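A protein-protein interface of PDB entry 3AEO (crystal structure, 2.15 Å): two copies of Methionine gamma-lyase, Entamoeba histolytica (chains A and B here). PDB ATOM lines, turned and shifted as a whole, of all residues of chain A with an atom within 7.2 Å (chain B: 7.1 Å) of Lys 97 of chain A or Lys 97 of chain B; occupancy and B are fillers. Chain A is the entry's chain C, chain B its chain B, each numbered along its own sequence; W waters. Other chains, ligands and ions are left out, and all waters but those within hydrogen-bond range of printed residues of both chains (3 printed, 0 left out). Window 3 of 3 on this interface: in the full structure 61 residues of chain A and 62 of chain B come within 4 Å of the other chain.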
ATOM      1  N   PHE A  94      14.756   8.242 -12.042  1.00  0.00           N
ATOM      2  CA  PHE A  94      14.932   8.951 -13.325  1.00  0.00           C
ATOM      3  C   PHE A  94      16.028   8.389 -14.239  1.00  0.00           C
ATOM      4  O   PHE A  94      15.913   8.478 -15.445  1.00  0.00           O
ATOM      5  CB  PHE A  94      15.200  10.439 -13.098  1.00  0.00           C
ATOM      6  CG  PHE A  94      14.210  11.089 -12.157  1.00  0.00           C
ATOM      7  CD1 PHE A  94      14.521  11.240 -10.824  1.00  0.00           C
ATOM      8  CD2 PHE A  94      12.967  11.516 -12.620  1.00  0.00           C
ATOM      9  CE1 PHE A  94      13.617  11.812  -9.959  1.00  0.00           C
ATOM     10  CE2 PHE A  94      12.074  12.112 -11.770  1.00  0.00           C
ATOM     11  CZ  PHE A  94      12.383  12.238 -10.432  1.00  0.00           C
ATOM     12  N   LEU A  95      17.095   7.831 -13.674  1.00  0.00           N
ATOM     13  CA  LEU A  95      18.212   7.377 -14.502  1.00  0.00           C
ATOM     14  C   LEU A  95      17.917   5.990 -15.007  1.00  0.00           C
ATOM     15  O   LEU A  95      17.422   5.146 -14.262  1.00  0.00           O
ATOM     16  CB  LEU A  95      19.525   7.362 -13.695  1.00  0.00           C
ATOM     17  CG  LEU A  95      20.004   8.738 -13.197  1.00  0.00           C
ATOM     18  CD1 LEU A  95      21.048   8.518 -12.138  1.00  0.00           C
ATOM     19  CD2 LEU A  95      20.588   9.579 -14.373  1.00  0.00           C
ATOM     20  N   GLN A  96      18.202   5.746 -16.275  1.00  0.00           N
ATOM     21  CA  GLN A  96      18.057   4.416 -16.824  1.00  0.00           C
ATOM     22  C   GLN A  96      19.308   4.061 -17.633  1.00  0.00           C
ATOM     23  O   GLN A  96      20.179   4.890 -17.824  1.00  0.00           O
ATOM     24  CB  GLN A  96      16.779   4.331 -17.698  1.00  0.00           C
ATOM     25  CG  GLN A  96      16.875   5.046 -19.006  1.00  0.00           C
ATOM     26  CD  GLN A  96      15.539   5.104 -19.729  1.00  0.00           C
ATOM     27  OE1 GLN A  96      15.086   4.114 -20.288  1.00  0.00           O
ATOM     28  NE2 GLN A  96      14.895   6.262 -19.691  1.00  0.00           N
ATOM     29  N   LYS A  97      19.388   2.815 -18.091  1.00  0.00           N
ATOM     30  CA  LYS A  97      20.506   2.325 -18.872  1.00  0.00           C
ATOM     31  C   LYS A  97      20.847   3.288 -20.043  1.00  0.00           C
ATOM     32  O   LYS A  97      19.963   3.715 -20.806  1.00  0.00           O
ATOM     33  CB  LYS A  97      20.149   0.935 -19.415  1.00  0.00           C
ATOM     34  CG  LYS A  97      21.211   0.277 -20.312  1.00  0.00           C
ATOM     35  CD  LYS A  97      20.600  -0.936 -21.049  1.00  0.00           C
ATOM     36  CE  LYS A  97      21.379  -1.351 -22.316  1.00  0.00           C
ATOM     37  NZ  LYS A  97      20.573  -2.353 -23.127  1.00  0.00           N
ATOM     38  N   GLY A  98      22.128   3.620 -20.186  1.00  0.00           N
ATOM     39  CA  GLY A  98      22.541   4.548 -21.242  1.00  0.00           C
ATOM     40  C   GLY A  98      22.674   6.001 -20.754  1.00  0.00           C
ATOM     41  O   GLY A  98      23.305   6.810 -21.442  1.00  0.00           O
ATOM     42  N   ASP A  99      22.073   6.338 -19.601  1.00  0.00           N
ATOM     43  CA  ASP A  99      22.188   7.686 -19.010  1.00  0.00           C
ATOM     44  C   ASP A  99      23.526   7.882 -18.288  1.00  0.00           C
ATOM     45  O   ASP A  99      24.161   6.901 -17.842  1.00  0.00           O
ATOM     46  CB  ASP A  99      21.052   7.935 -17.984  1.00  0.00           C
ATOM     47  CG  ASP A  99      19.676   8.129 -18.662  1.00  0.00           C
ATOM     48  OD1 ASP A  99      18.626   8.122 -17.977  1.00  0.00           O
ATOM     49  OD2 ASP A  99      19.639   8.296 -19.885  1.00  0.00           O
ATOM     50  N   HIS A 100      23.907   9.145 -18.099  1.00  0.00           N
ATOM     51  CA  HIS A 100      25.160   9.502 -17.413  1.00  0.00           C
ATOM     52  C   HIS A 100      24.865  10.383 -16.226  1.00  0.00           C
ATOM     53  O   HIS A 100      24.067  11.365 -16.307  1.00  0.00           O
ATOM     54  CB  HIS A 100      26.126  10.161 -18.413  1.00  0.00           C
ATOM     55  CG  HIS A 100      27.343  10.797 -17.814  1.00  0.00           C
ATOM     56  ND1 HIS A 100      28.365  10.072 -17.218  1.00  0.00           N
ATOM     57  CD2 HIS A 100      27.757  12.082 -17.825  1.00  0.00           C
ATOM     58  CE1 HIS A 100      29.329  10.891 -16.839  1.00  0.00           C
ATOM     59  NE2 HIS A 100      28.984  12.119 -17.203  1.00  0.00           N
ATOM     60  N   LEU A 119      24.636   1.347  -9.491  1.00  0.00           N
ATOM     61  CA  LEU A 119      24.240   1.988 -10.739  1.00  0.00           C
ATOM     62  C   LEU A 119      24.879   1.414 -12.010  1.00  0.00           C
ATOM     63  O   LEU A 119      24.164   1.220 -12.992  1.00  0.00           O
ATOM     64  CB  LEU A 119      24.442   3.500 -10.714  1.00  0.00           C
ATOM     65  CG  LEU A 119      23.727   4.433  -9.745  1.00  0.00           C
ATOM     66  CD1 LEU A 119      23.390   5.791 -10.398  1.00  0.00           C
ATOM     67  CD2 LEU A 119      22.576   3.854  -8.855  1.00  0.00           C
ATOM     68  N   PRO A 120      26.215   1.129 -11.998  1.00  0.00           N
ATOM     69  CA  PRO A 120      26.832   0.561 -13.194  1.00  0.00           C
ATOM     70  C   PRO A 120      26.254  -0.793 -13.543  1.00  0.00           C
ATOM     71  O   PRO A 120      26.187  -1.138 -14.719  1.00  0.00           O
ATOM     72  CB  PRO A 120      28.307   0.412 -12.812  1.00  0.00           C
ATOM     73  CG  PRO A 120      28.508   1.526 -11.781  1.00  0.00           C
ATOM     74  CD  PRO A 120      27.226   1.541 -11.006  1.00  0.00           C
ATOM     75  N   ARG A 121      25.826  -1.546 -12.534  1.00  0.00           N
ATOM     76  CA  ARG A 121      25.186  -2.833 -12.777  1.00  0.00           C
ATOM     77  C   ARG A 121      23.868  -2.658 -13.527  1.00  0.00           C
ATOM     78  O   ARG A 121      23.428  -3.577 -14.224  1.00  0.00           O
ATOM     79  CB  ARG A 121      24.954  -3.576 -11.471  1.00  0.00           C
ATOM     80  CG  ARG A 121      26.211  -4.147 -10.880  1.00  0.00           C
ATOM     81  CD  ARG A 121      25.980  -4.700  -9.455  1.00  0.00           C
ATOM     82  NE  ARG A 121      25.147  -5.911  -9.403  1.00  0.00           N
ATOM     83  CZ  ARG A 121      25.578  -7.163  -9.605  1.00  0.00           C
ATOM     84  NH1 ARG A 121      26.843  -7.427  -9.905  1.00  0.00           N
ATOM     85  NH2 ARG A 121      24.722  -8.161  -9.524  1.00  0.00           N
ATOM     86  N   PHE A 122      23.279  -1.460 -13.423  1.00  0.00           N
ATOM     87  CA  PHE A 122      22.029  -1.154 -14.128  1.00  0.00           C
ATOM     88  C   PHE A 122      22.195  -0.396 -15.438  1.00  0.00           C
ATOM     89  O   PHE A 122      21.207   0.080 -15.993  1.00  0.00           O
ATOM     90  CB  PHE A 122      21.040  -0.416 -13.195  1.00  0.00           C
ATOM     91  CG  PHE A 122      20.764  -1.160 -11.894  1.00  0.00           C
ATOM     92  CD1 PHE A 122      20.593  -0.468 -10.707  1.00  0.00           C
ATOM     93  CD2 PHE A 122      20.711  -2.556 -11.862  1.00  0.00           C
ATOM     94  CE1 PHE A 122      20.367  -1.144  -9.512  1.00  0.00           C
ATOM     95  CE2 PHE A 122      20.484  -3.230 -10.658  1.00  0.00           C
ATOM     96  CZ  PHE A 122      20.299  -2.509  -9.481  1.00  0.00           C
ATOM     97  N   GLY A 123      23.430  -0.290 -15.934  1.00  0.00           N
ATOM     98  CA  GLY A 123      23.716   0.297 -17.252  1.00  0.00           C
ATOM     99  C   GLY A 123      23.905   1.809 -17.153  1.00  0.00           C
ATOM    100  O   GLY A 123      23.957   2.505 -18.174  1.00  0.00           O
ATOM    101  N   ILE A 124      24.004   2.333 -15.926  1.00  0.00           N
ATOM    102  CA  ILE A 124      24.135   3.787 -15.758  1.00  0.00           C
ATOM    103  C   ILE A 124      25.609   4.149 -15.645  1.00  0.00           C
ATOM    104  O   ILE A 124      26.345   3.487 -14.923  1.00  0.00           O
ATOM    105  CB  ILE A 124      23.322   4.285 -14.536  1.00  0.00           C
ATOM    106  CG1 ILE A 124      21.830   3.995 -14.753  1.00  0.00           C
ATOM    107  CG2 ILE A 124      23.546   5.805 -14.264  1.00  0.00           C
ATOM    108  CD1 ILE A 124      21.026   3.860 -13.438  1.00  0.00           C
ATOM    109  N   GLU A 125      26.046   5.166 -16.389  1.00  0.00           N
ATOM    110  CA  GLU A 125      27.444   5.582 -16.400  1.00  0.00           C
ATOM    111  C   GLU A 125      27.563   6.653 -15.347  1.00  0.00           C
ATOM    112  O   GLU A 125      26.708   7.531 -15.260  1.00  0.00           O
ATOM    113  CB  GLU A 125      27.862   6.137 -17.791  1.00  0.00           C
ATOM    114  CG  GLU A 125      27.657   5.168 -18.973  1.00  0.00           C
ATOM    115  CD  GLU A 125      27.644   5.831 -20.391  1.00  0.00           C
ATOM    116  OE1 GLU A 125      27.739   7.070 -20.554  1.00  0.00           O
ATOM    117  OE2 GLU A 125      27.517   5.078 -21.377  1.00  0.00           O
ATOM    118  N   ASN A 144      24.838  12.494 -23.180  1.00  0.00           N
ATOM    119  CA  ASN A 144      23.871  11.694 -22.395  1.00  0.00           C
ATOM    120  C   ASN A 144      23.841  12.019 -20.867  1.00  0.00           C
ATOM    121  O   ASN A 144      23.242  11.281 -20.088  1.00  0.00           O
ATOM    122  CB  ASN A 144      24.115  10.184 -22.653  1.00  0.00           C
ATOM    123  CG  ASN A 144      25.501   9.704 -22.134  1.00  0.00           C
ATOM    124  OD1 ASN A 144      26.512  10.410 -22.257  1.00  0.00           O
ATOM    125  ND2 ASN A 144      25.543   8.497 -21.574  1.00  0.00           N
ATOM    126  N   LEU B  95      20.343  -9.524 -10.147  1.00  0.00           N
ATOM    127  CA  LEU B  95      20.188  -9.247 -11.561  1.00  0.00           C
ATOM    128  C   LEU B  95      20.924  -7.970 -11.936  1.00  0.00           C
ATOM    129  O   LEU B  95      20.926  -6.991 -11.175  1.00  0.00           O
ATOM    130  CB  LEU B  95      18.721  -9.114 -11.923  1.00  0.00           C
ATOM    131  CG  LEU B  95      17.893 -10.373 -11.689  1.00  0.00           C
ATOM    132  CD1 LEU B  95      16.409 -10.054 -11.819  1.00  0.00           C
ATOM    133  CD2 LEU B  95      18.302 -11.481 -12.614  1.00  0.00           C
ATOM    134  N   GLN B  96      21.577  -8.008 -13.095  1.00  0.00           N
ATOM    135  CA  GLN B  96      22.223  -6.838 -13.678  1.00  0.00           C
ATOM    136  C   GLN B  96      21.990  -6.797 -15.196  1.00  0.00           C
ATOM    137  O   GLN B  96      21.483  -7.763 -15.788  1.00  0.00           O
ATOM    138  CB  GLN B  96      23.721  -6.812 -13.339  1.00  0.00           C
ATOM    139  CG  GLN B  96      24.563  -7.831 -14.064  1.00  0.00           C
ATOM    140  CD  GLN B  96      25.976  -7.908 -13.528  1.00  0.00           C
ATOM    141  OE1 GLN B  96      26.753  -6.954 -13.616  1.00  0.00           O
ATOM    142  NE2 GLN B  96      26.328  -9.069 -12.988  1.00  0.00           N
ATOM    143  N   LYS B  97      22.344  -5.664 -15.801  1.00  0.00           N
ATOM    144  CA  LYS B  97      22.149  -5.423 -17.222  1.00  0.00           C
ATOM    145  C   LYS B  97      22.664  -6.616 -18.025  1.00  0.00           C
ATOM    146  O   LYS B  97      23.778  -7.074 -17.798  1.00  0.00           O
ATOM    147  CB  LYS B  97      22.873  -4.135 -17.619  1.00  0.00           C
ATOM    148  CG  LYS B  97      23.082  -3.921 -19.112  1.00  0.00           C
ATOM    149  CD  LYS B  97      24.011  -2.718 -19.341  1.00  0.00           C
ATOM    150  CE  LYS B  97      24.677  -2.709 -20.757  1.00  0.00           C
ATOM    151  NZ  LYS B  97      25.548  -1.486 -20.947  1.00  0.00           N
ATOM    152  N   GLY B  98      21.839  -7.118 -18.939  1.00  0.00           N
ATOM    153  CA  GLY B  98      22.210  -8.291 -19.750  1.00  0.00           C
ATOM    154  C   GLY B  98      21.714  -9.624 -19.216  1.00  0.00           C
ATOM    155  O   GLY B  98      21.794 -10.644 -19.927  1.00  0.00           O
ATOM    156  N   ASP B  99      21.233  -9.636 -17.964  1.00  0.00           N
ATOM    157  CA  ASP B  99      20.593 -10.820 -17.384  1.00  0.00           C
ATOM    158  C   ASP B  99      19.150 -10.951 -17.877  1.00  0.00           C
ATOM    159  O   ASP B  99      18.552  -9.977 -18.345  1.00  0.00           O
ATOM    160  CB  ASP B  99      20.631 -10.816 -15.848  1.00  0.00           C
ATOM    161  CG  ASP B  99      22.050 -10.945 -15.280  1.00  0.00           C
ATOM    162  OD1 ASP B  99      22.283 -10.553 -14.101  1.00  0.00           O
ATOM    163  OD2 ASP B  99      22.950 -11.420 -15.992  1.00  0.00           O
ATOM    164  N   HIS B 100      18.608 -12.160 -17.756  1.00  0.00           N
ATOM    165  CA  HIS B 100      17.238 -12.482 -18.146  1.00  0.00           C
ATOM    166  C   HIS B 100      16.502 -13.120 -16.969  1.00  0.00           C
ATOM    167  O   HIS B 100      17.053 -13.968 -16.252  1.00  0.00           O
ATOM    168  CB  HIS B 100      17.292 -13.436 -19.344  1.00  0.00           C
ATOM    169  CG  HIS B 100      15.971 -14.048 -19.736  1.00  0.00           C
ATOM    170  ND1 HIS B 100      14.877 -13.300 -20.128  1.00  0.00           N
ATOM    171  CD2 HIS B 100      15.605 -15.346 -19.886  1.00  0.00           C
ATOM    172  CE1 HIS B 100      13.884 -14.112 -20.459  1.00  0.00           C
ATOM    173  NE2 HIS B 100      14.302 -15.357 -20.326  1.00  0.00           N
ATOM    174  N   LEU B 119      12.728  -2.967 -14.031  1.00  0.00           N
ATOM    175  CA  LEU B 119      13.798  -3.889 -14.482  1.00  0.00           C
ATOM    176  C   LEU B 119      14.259  -3.667 -15.930  1.00  0.00           C
ATOM    177  O   LEU B 119      15.447  -3.683 -16.171  1.00  0.00           O
ATOM    178  CB  LEU B 119      13.430  -5.377 -14.315  1.00  0.00           C
ATOM    179  CG  LEU B 119      13.135  -5.984 -12.947  1.00  0.00           C
ATOM    180  CD1 LEU B 119      13.632  -7.420 -12.853  1.00  0.00           C
ATOM    181  CD2 LEU B 119      13.575  -5.160 -11.732  1.00  0.00           C
ATOM    182  N   PRO B 120      13.329  -3.453 -16.889  1.00  0.00           N
ATOM    183  CA  PRO B 120      13.832  -3.201 -18.255  1.00  0.00           C
ATOM    184  C   PRO B 120      14.618  -1.898 -18.422  1.00  0.00           C
ATOM    185  O   PRO B 120      15.455  -1.802 -19.325  1.00  0.00           O
ATOM    186  CB  PRO B 120      12.556  -3.192 -19.128  1.00  0.00           C
ATOM    187  CG  PRO B 120      11.559  -3.960 -18.359  1.00  0.00           C
ATOM    188  CD  PRO B 120      11.863  -3.612 -16.887  1.00  0.00           C
ATOM    189  N   ARG B 121      14.342  -0.904 -17.580  1.00  0.00           N
ATOM    190  CA  ARG B 121      15.082   0.350 -17.589  1.00  0.00           C
ATOM    191  C   ARG B 121      16.521   0.129 -17.102  1.00  0.00           C
ATOM    192  O   ARG B 121      17.443   0.868 -17.481  1.00  0.00           O
ATOM    193  CB  ARG B 121      14.378   1.383 -16.695  1.00  0.00           C
ATOM    194  CG  ARG B 121      13.066   1.941 -17.300  1.00  0.00           C
ATOM    195  CD  ARG B 121      12.262   2.758 -16.251  1.00  0.00           C
ATOM    196  NE  ARG B 121      12.910   4.005 -15.881  1.00  0.00           N
ATOM    197  CZ  ARG B 121      12.798   5.150 -16.545  1.00  0.00           C
ATOM    198  NH1 ARG B 121      13.455   6.224 -16.117  1.00  0.00           N
ATOM    199  NH2 ARG B 121      12.029   5.231 -17.629  1.00  0.00           N
ATOM    200  N   PHE B 122      16.710  -0.878 -16.256  1.00  0.00           N
ATOM    201  CA  PHE B 122      18.058  -1.236 -15.798  1.00  0.00           C
ATOM    202  C   PHE B 122      18.764  -2.307 -16.680  1.00  0.00           C
ATOM    203  O   PHE B 122      19.787  -2.863 -16.285  1.00  0.00           O
ATOM    204  CB  PHE B 122      18.030  -1.656 -14.325  1.00  0.00           C
ATOM    205  CG  PHE B 122      17.307  -0.685 -13.427  1.00  0.00           C
ATOM    206  CD1 PHE B 122      16.536  -1.147 -12.378  1.00  0.00           C
ATOM    207  CD2 PHE B 122      17.411   0.687 -13.619  1.00  0.00           C
ATOM    208  CE1 PHE B 122      15.864  -0.237 -11.495  1.00  0.00           C
ATOM    209  CE2 PHE B 122      16.743   1.606 -12.763  1.00  0.00           C
ATOM    210  CZ  PHE B 122      15.958   1.124 -11.698  1.00  0.00           C
ATOM    211  N   GLY B 123      18.205  -2.579 -17.862  1.00  0.00           N
ATOM    212  CA  GLY B 123      18.836  -3.489 -18.845  1.00  0.00           C
ATOM    213  C   GLY B 123      18.578  -4.961 -18.586  1.00  0.00           C
ATOM    214  O   GLY B 123      19.250  -5.814 -19.138  1.00  0.00           O
ATOM    215  N   ILE B 124      17.607  -5.258 -17.723  1.00  0.00           N
ATOM    216  CA  ILE B 124      17.239  -6.643 -17.426  1.00  0.00           C
ATOM    217  C   ILE B 124      16.039  -7.087 -18.268  1.00  0.00           C
ATOM    218  O   ILE B 124      14.996  -6.420 -18.257  1.00  0.00           O
ATOM    219  CB  ILE B 124      16.967  -6.832 -15.915  1.00  0.00           C
ATOM    220  CG1 ILE B 124      18.225  -6.460 -15.105  1.00  0.00           C
ATOM    221  CG2 ILE B 124      16.535  -8.272 -15.607  1.00  0.00           C
ATOM    222  CD1 ILE B 124      17.922  -5.968 -13.672  1.00  0.00           C
ATOM    223  N   GLU B 125      16.200  -8.201 -18.992  1.00  0.00           N
ATOM    224  CA  GLU B 125      15.136  -8.763 -19.822  1.00  0.00           C
ATOM    225  C   GLU B 125      14.220  -9.620 -18.976  1.00  0.00           C
ATOM    226  O   GLU B 125      14.680 -10.457 -18.198  1.00  0.00           O
ATOM    227  CB  GLU B 125      15.691  -9.621 -20.973  1.00  0.00           C
ATOM    228  CG  GLU B 125      16.975  -9.099 -21.625  1.00  0.00           C
ATOM    229  CD  GLU B 125      17.700 -10.152 -22.495  1.00  0.00           C
ATOM    230  OE1 GLU B 125      17.125 -11.215 -22.810  1.00  0.00           O
ATOM    231  OE2 GLU B 125      18.867  -9.909 -22.865  1.00  0.00           O
HETATM  232  O   HOH W   1      14.769   4.765 -13.918  1.00  0.00           O
HETATM  233  O   HOH W   2      22.313  -6.277  -9.266  1.00  0.00           O
HETATM  234  O   HOH W   3      13.124   9.146 -17.015  1.00  0.00           O
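Leu 95 of chain A touches Phe 122 of chain B, and with the chains exchanged Phe 122 of chain A touches Leu 95 of chain B. Lys 97 of chain A touches Arg 121 of chain B, and with the chains exchanged Arg 121 of chain A touches Lys 97 of chain B. Lys 97 of chain A touches Gly 123 of chain B, and with the chains exchanged Gly 123 of chain A touches Lys 97 of chain B. Phe 122 of chain B touches its own counterpart, Phe 122 of chain A. 13 positions are printed for both chains.
Leu 95 of chain A touches Phe 122 of chain B (O to CE2, 3.9 Å). O of Arg 121 of chain B touches CB of Gln 96 of chain A (3.5 Å). CE of Lys 97 of chain B touches CE of Lys 97 of chain A (3.9 Å). Lys 97 of chain A touches Gly 123 of chain B. Gln 96 of chain B touches Arg 121 of chain A (CB to O, 3.4 Å). Leu 95 of chain B touches Phe 122 of chain A. Gly 123 of chain A touches Lys 97 of chain B (CA to CD, 3.7 Å).
The backbone NH (N) of Lys 97 of chain B is in hydrogen-bond range of the backbone carbonyl oxygen (O) of Arg 121 of chain A. The backbone carbonyl oxygen (O) of Phe 122 of chain A sits close to the backbone carbonyl oxygen (O) of Phe 122 of chain B (3.3 Å). The backbone NH (N) of Lys 97 of chain A lies within hydrogen-bond range of the backbone carbonyl oxygen (O) of Arg 121 of chain B. The backbone carbonyl oxygen (O) of Phe 94 of chain A lies within hydrogen-bond range of the guanidinium group (NH1) of Arg 121 of chain B (3.4 Å).
Hydrophobic or aromatic side chains of chain A that line the printed part of chain B: Phe 122. Printed residues of chain B that touch a printed residue of chain A: Leu 95, Gln 96, Lys 97, Arg 121, Phe 122 and Gly 123. Among the printed residues, no Asp or Glu carboxylate lies within 4 Å of a Lys or Arg side-chain nitrogen of the other chain.
N of Gly 98 of chain A is in hydrogen-bond range of O of Gly 123 of chain A (2.9 Å). The backbone NH (N) of Gln 96 of chain B is in hydrogen-bond range of the side-chain carboxylate (OD1) of Asp 99 of chain B, at 2.8 Å. N of Gln 96 of chain A sits at hydrogen-bond distance from OD1 of Asp 99 of chain A, 3.0 Å away. The backbone NH (N) of Gly 98 of chain B lies within hydrogen-bond range of the backbone carbonyl oxygen (O) of Gly 123 of chain B, 2.9 Å away.
Of the printed residues of chain B, Phe 94 of chain A touches Arg 121 (3.4 Å). Of the printed residues of chain B, Leu 95 of chain A touches Phe 122 (3.9 Å). Of chain B, only Lys 97, Arg 121 and Gly 123 come within 4 Å of Lys 97 of chain A. Of the printed residues of chain B, Arg 121 of chain A touches Gln 96 (3.4 Å) and Lys 97 (2.8 Å). Of the printed residues of chain A, Leu 95 of chain B touches Phe 122. Of the printed residues of chain A, Gln 96 of chain B touches Arg 121. Asp 99 of chain B touches none of the printed residues of chain A. The nearest printed residue of chain B that does not touch Gln 96 of chain A is Phe 122 of chain B (5.0 Å).
Water W2 lies within hydrogen-bond range of the backbone carbonyl oxygen of Leu 95 of chain B (2.5 Å) and the guanidinium group of Arg 121 of chain A (2.9 Å). Water W1 lies within hydrogen-bond range of the backbone carbonyl oxygen (O) of Leu 95 of chain A (2.7 Å) and the guanidinium group (NE) of Arg 121 of chain B (2.8 Å). Water W3 lies within hydrogen-bond range of NH1 of Arg 121 of chain B (3.1 Å) and O of Phe 94 of chain A (3.3 Å).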
